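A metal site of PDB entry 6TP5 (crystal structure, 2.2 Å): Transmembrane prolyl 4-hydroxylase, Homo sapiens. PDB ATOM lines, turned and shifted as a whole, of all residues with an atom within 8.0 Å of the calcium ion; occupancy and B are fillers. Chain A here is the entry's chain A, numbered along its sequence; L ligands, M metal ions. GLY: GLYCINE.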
ATOM      1  N   PHE A 113     -17.539 -37.265 -11.882  1.00  0.00           N
ATOM      2  CA  PHE A 113     -17.736 -35.861 -12.226  1.00  0.00           C
ATOM      3  C   PHE A 113     -16.702 -35.398 -13.250  1.00  0.00           C
ATOM      4  O   PHE A 113     -17.059 -34.832 -14.286  1.00  0.00           O
ATOM      5  CB  PHE A 113     -17.673 -34.996 -10.966  1.00  0.00           C
ATOM      6  CG  PHE A 113     -18.060 -33.559 -11.196  1.00  0.00           C
ATOM      7  CD1 PHE A 113     -17.122 -32.624 -11.602  1.00  0.00           C
ATOM      8  CD2 PHE A 113     -19.375 -33.158 -11.019  1.00  0.00           C
ATOM      9  CE1 PHE A 113     -17.488 -31.302 -11.818  1.00  0.00           C
ATOM     10  CE2 PHE A 113     -19.736 -31.829 -11.224  1.00  0.00           C
ATOM     11  CZ  PHE A 113     -18.802 -30.910 -11.637  1.00  0.00           C
ATOM     12  N   LEU A 116     -17.578 -36.672 -16.628  1.00  0.00           N
ATOM     13  CA  LEU A 116     -18.733 -36.039 -17.258  1.00  0.00           C
ATOM     14  C   LEU A 116     -18.460 -34.592 -17.661  1.00  0.00           C
ATOM     15  O   LEU A 116     -18.980 -34.129 -18.679  1.00  0.00           O
ATOM     16  CB  LEU A 116     -19.944 -36.097 -16.325  1.00  0.00           C
ATOM     17  CG  LEU A 116     -20.343 -37.487 -15.820  1.00  0.00           C
ATOM     18  CD1 LEU A 116     -21.666 -37.438 -15.092  1.00  0.00           C
ATOM     19  CD2 LEU A 116     -20.411 -38.458 -16.976  1.00  0.00           C
ATOM     20  N   ASP A 117     -17.645 -33.863 -16.887  1.00  0.00           N
ATOM     21  CA  ASP A 117     -17.401 -32.443 -17.136  1.00  0.00           C
ATOM     22  C   ASP A 117     -16.400 -32.309 -18.288  1.00  0.00           C
ATOM     23  O   ASP A 117     -15.209 -32.056 -18.100  1.00  0.00           O
ATOM     24  CB  ASP A 117     -16.896 -31.765 -15.872  1.00  0.00           C
ATOM     25  CG  ASP A 117     -16.791 -30.254 -16.016  1.00  0.00           C
ATOM     26  OD1 ASP A 117     -17.216 -29.729 -17.071  1.00  0.00           O
ATOM     27  OD2 ASP A 117     -16.271 -29.589 -15.092  1.00  0.00           O
ATOM     28  N   GLN A 118     -16.918 -32.459 -19.510  1.00  0.00           N
ATOM     29  CA  GLN A 118     -16.071 -32.423 -20.701  1.00  0.00           C
ATOM     30  C   GLN A 118     -15.328 -31.098 -20.823  1.00  0.00           C
ATOM     31  O   GLN A 118     -14.107 -31.074 -21.006  1.00  0.00           O
ATOM     32  CB  GLN A 118     -16.913 -32.676 -21.954  1.00  0.00           C
ATOM     33  CG  GLN A 118     -17.251 -34.122 -22.219  1.00  0.00           C
ATOM     34  CD  GLN A 118     -18.009 -34.299 -23.522  1.00  0.00           C
ATOM     35  OE1 GLN A 118     -19.200 -34.631 -23.529  1.00  0.00           O
ATOM     36  NE2 GLN A 118     -17.315 -34.089 -24.641  1.00  0.00           N
ATOM     37  N   ASN A 119     -16.047 -29.984 -20.736  1.00  0.00           N
ATOM     38  CA  ASN A 119     -15.429 -28.669 -20.933  1.00  0.00           C
ATOM     39  C   ASN A 119     -14.746 -28.142 -19.678  1.00  0.00           C
ATOM     40  O   ASN A 119     -14.216 -27.017 -19.717  1.00  0.00           O
ATOM     41  CB  ASN A 119     -16.467 -27.671 -21.454  1.00  0.00           C
ATOM     42  CG  ASN A 119     -17.465 -27.238 -20.390  1.00  0.00           C
ATOM     43  OD1 ASN A 119     -17.608 -27.893 -19.353  1.00  0.00           O
ATOM     44  ND2 ASN A 119     -18.174 -26.145 -20.654  1.00  0.00           N
ATOM     45  N   ARG A 120     -14.739 -28.906 -18.585  1.00  0.00           N
ATOM     46  CA  ARG A 120     -13.903 -28.639 -17.414  1.00  0.00           C
ATOM     47  C   ARG A 120     -14.171 -27.251 -16.817  1.00  0.00           C
ATOM     48  O   ARG A 120     -13.257 -26.506 -16.482  1.00  0.00           O
ATOM     49  CB  ARG A 120     -12.419 -28.800 -17.740  1.00  0.00           C
ATOM     50  CG  ARG A 120     -12.065 -30.042 -18.538  1.00  0.00           C
ATOM     51  CD  ARG A 120     -10.561 -30.100 -18.800  1.00  0.00           C
ATOM     52  NE  ARG A 120     -10.123 -29.052 -19.719  1.00  0.00           N
ATOM     53  CZ  ARG A 120      -8.954 -29.043 -20.361  1.00  0.00           C
ATOM     54  NH1 ARG A 120      -8.644 -28.045 -21.167  1.00  0.00           N
ATOM     55  NH2 ARG A 120      -8.097 -30.037 -20.183  1.00  0.00           N
ATOM     56  N   ASP A 121     -15.454 -26.915 -16.667  1.00  0.00           N
ATOM     57  CA  ASP A 121     -15.819 -25.654 -16.028  1.00  0.00           C
ATOM     58  C   ASP A 121     -16.416 -25.862 -14.640  1.00  0.00           C
ATOM     59  O   ASP A 121     -17.021 -24.934 -14.081  1.00  0.00           O
ATOM     60  CB  ASP A 121     -16.768 -24.849 -16.928  1.00  0.00           C
ATOM     61  CG  ASP A 121     -18.116 -25.509 -17.118  1.00  0.00           C
ATOM     62  OD1 ASP A 121     -18.308 -26.656 -16.657  1.00  0.00           O
ATOM     63  OD2 ASP A 121     -18.996 -24.887 -17.753  1.00  0.00           O
ATOM     64  N   GLY A 122     -16.273 -27.058 -14.075  1.00  0.00           N
ATOM     65  CA  GLY A 122     -16.772 -27.335 -12.736  1.00  0.00           C
ATOM     66  C   GLY A 122     -18.270 -27.473 -12.640  1.00  0.00           C
ATOM     67  O   GLY A 122     -18.812 -27.453 -11.528  1.00  0.00           O
ATOM     68  N   HIS A 123     -18.959 -27.613 -13.776  1.00  0.00           N
ATOM     69  CA  HIS A 123     -20.404 -27.698 -13.832  1.00  0.00           C
ATOM     70  C   HIS A 123     -20.800 -28.741 -14.865  1.00  0.00           C
ATOM     71  O   HIS A 123     -20.213 -28.788 -15.953  1.00  0.00           O
ATOM     72  CB  HIS A 123     -21.025 -26.341 -14.201  1.00  0.00           C
ATOM     73  CG  HIS A 123     -20.864 -25.279 -13.157  1.00  0.00           C
ATOM     74  ND1 HIS A 123     -19.662 -24.662 -12.904  1.00  0.00           N
ATOM     75  CD2 HIS A 123     -21.761 -24.720 -12.315  1.00  0.00           C
ATOM     76  CE1 HIS A 123     -19.818 -23.765 -11.946  1.00  0.00           C
ATOM     77  NE2 HIS A 123     -21.082 -23.786 -11.569  1.00  0.00           N
ATOM     78  N   LEU A 124     -21.785 -29.566 -14.520  1.00  0.00           N
ATOM     79  CA  LEU A 124     -22.341 -30.539 -15.463  1.00  0.00           C
ATOM     80  C   LEU A 124     -23.508 -29.890 -16.191  1.00  0.00           C
ATOM     81  O   LEU A 124     -24.599 -29.736 -15.628  1.00  0.00           O
ATOM     82  CB  LEU A 124     -22.784 -31.812 -14.741  1.00  0.00           C
ATOM     83  CG  LEU A 124     -21.680 -32.609 -14.042  1.00  0.00           C
ATOM     84  CD1 LEU A 124     -22.158 -34.010 -13.672  1.00  0.00           C
ATOM     85  CD2 LEU A 124     -20.431 -32.673 -14.913  1.00  0.00           C
ATOM     86  N   GLN A 125     -23.280 -29.513 -17.439  1.00  0.00           N
ATOM     87  CA  GLN A 125     -24.375 -29.066 -18.295  1.00  0.00           C
ATOM     88  C   GLN A 125     -25.229 -30.264 -18.715  1.00  0.00           C
ATOM     89  O   GLN A 125     -24.819 -31.421 -18.608  1.00  0.00           O
ATOM     90  CB  GLN A 125     -23.826 -28.347 -19.533  1.00  0.00           C
ATOM     91  CG  GLN A 125     -23.336 -26.932 -19.258  1.00  0.00           C
ATOM     92  CD  GLN A 125     -21.912 -26.859 -18.709  1.00  0.00           C
ATOM     93  OE1 GLN A 125     -21.115 -27.776 -18.876  1.00  0.00           O
ATOM     94  NE2 GLN A 125     -21.585 -25.744 -18.049  1.00  0.00           N
ATOM     95  N   LEU A 126     -26.448 -29.973 -19.180  1.00  0.00           N
ATOM     96  CA  LEU A 126     -27.333 -31.038 -19.662  1.00  0.00           C
ATOM     97  C   LEU A 126     -26.664 -31.844 -20.775  1.00  0.00           C
ATOM     98  O   LEU A 126     -26.724 -33.084 -20.774  1.00  0.00           O
ATOM     99  CB  LEU A 126     -28.655 -30.452 -20.142  1.00  0.00           C
ATOM    100  CG  LEU A 126     -29.589 -29.956 -19.036  1.00  0.00           C
ATOM    101  CD1 LEU A 126     -30.812 -29.238 -19.594  1.00  0.00           C
ATOM    102  CD2 LEU A 126     -30.005 -31.105 -18.146  1.00  0.00           C
ATOM    103  N   ARG A 127     -26.028 -31.167 -21.741  1.00  0.00           N
ATOM    104  CA  ARG A 127     -25.405 -31.875 -22.848  1.00  0.00           C
ATOM    105  C   ARG A 127     -24.319 -32.831 -22.369  1.00  0.00           C
ATOM    106  O   ARG A 127     -24.080 -33.873 -22.988  1.00  0.00           O
ATOM    107  CB  ARG A 127     -24.832 -30.882 -23.864  1.00  0.00           C
ATOM    108  CG  ARG A 127     -23.652 -30.032 -23.348  1.00  0.00           C
ATOM    109  CD  ARG A 127     -22.788 -29.435 -24.485  1.00  0.00           C
ATOM    110  NE  ARG A 127     -22.372 -30.429 -25.480  1.00  0.00           N
ATOM    111  CZ  ARG A 127     -21.452 -31.378 -25.276  1.00  0.00           C
ATOM    112  NH1 ARG A 127     -20.845 -31.503 -24.105  1.00  0.00           N
ATOM    113  NH2 ARG A 127     -21.158 -32.224 -26.256  1.00  0.00           N
ATOM    114  N   GLU A 128     -23.675 -32.518 -21.236  1.00  0.00           N
ATOM    115  CA  GLU A 128     -22.635 -33.398 -20.705  1.00  0.00           C
ATOM    116  C   GLU A 128     -23.233 -34.653 -20.062  1.00  0.00           C
ATOM    117  O   GLU A 128     -22.663 -35.739 -20.168  1.00  0.00           O
ATOM    118  CB  GLU A 128     -21.773 -32.645 -19.697  1.00  0.00           C
ATOM    119  CG  GLU A 128     -20.794 -31.674 -20.352  1.00  0.00           C
ATOM    120  CD  GLU A 128     -20.090 -30.803 -19.359  1.00  0.00           C
ATOM    121  OE1 GLU A 128     -20.597 -30.677 -18.226  1.00  0.00           O
ATOM    122  OE2 GLU A 128     -19.028 -30.229 -19.686  1.00  0.00           O
ATOM    123  N   VAL A 162     -28.278 -27.385 -14.338  1.00  0.00           N
ATOM    124  CA  VAL A 162     -26.835 -27.599 -14.224  1.00  0.00           C
ATOM    125  C   VAL A 162     -26.525 -28.086 -12.822  1.00  0.00           C
ATOM    126  O   VAL A 162     -27.010 -27.513 -11.837  1.00  0.00           O
ATOM    127  CB  VAL A 162     -26.061 -26.304 -14.547  1.00  0.00           C
ATOM    128  CG1 VAL A 162     -24.569 -26.519 -14.358  1.00  0.00           C
ATOM    129  CG2 VAL A 162     -26.396 -25.802 -15.957  1.00  0.00           C
ATOM    130  N   LEU A 163     -25.712 -29.134 -12.717  1.00  0.00           N
ATOM    131  CA  LEU A 163     -25.199 -29.594 -11.425  1.00  0.00           C
ATOM    132  C   LEU A 163     -23.783 -29.049 -11.257  1.00  0.00           C
ATOM    133  O   LEU A 163     -22.860 -29.477 -11.960  1.00  0.00           O
ATOM    134  CB  LEU A 163     -25.199 -31.112 -11.343  1.00  0.00           C
ATOM    135  CG  LEU A 163     -26.535 -31.839 -11.534  1.00  0.00           C
ATOM    136  CD1 LEU A 163     -26.302 -33.331 -11.351  1.00  0.00           C
ATOM    137  CD2 LEU A 163     -27.593 -31.317 -10.566  1.00  0.00           C
HETATM  138  N   GLY L   1     -20.497 -21.450 -16.429  1.00  0.00           N
HETATM  139  CA  GLY L   1     -21.126 -21.007 -15.197  1.00  0.00           C
HETATM  140  C   GLY L   1     -22.576 -21.430 -15.095  1.00  0.00           C
HETATM  141  O   GLY L   1     -23.191 -21.341 -14.029  1.00  0.00           O
HETATM  142  OXT GLY L   1     -23.185 -21.872 -16.068  1.00  0.00           O
HETATM  143 CA    CA M   1     -19.161 -28.594 -17.774  1.00  0.00          CA
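Of the 16 residues printed, 6 come within 4 Å of the calcium ion.
The calcium ion is bound by O of His 123 (2.1 Å), OD1 of Asn 119 (2.3 Å), OD1 of Asp 117 (2.4 Å), OE1 of Gln 125 (2.4 Å), OD1 of Asp 121 (2.4 Å), OE2 of Glu 128 (2.5 Å) and OE1 of Glu 128 (2.6 Å). The calcium ion has seven donor atoms within binding distance.
A nitrogen (N) of the ligand is in salt-bridge range of the side-chain carboxylate of Asp 121, at 3.98 Å.
The side-chain carboxylate (OE2) of Glu 128 lies close to the backbone NH (N) of Gln 118, 3.1 Å away. The side-chain carboxylate of Asp 117 lies within hydrogen-bond range of the backbone NH of Gly 122, at 2.7 Å. N of Arg 120 lies close to OD1 of Asp 117, at 3.0 Å.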
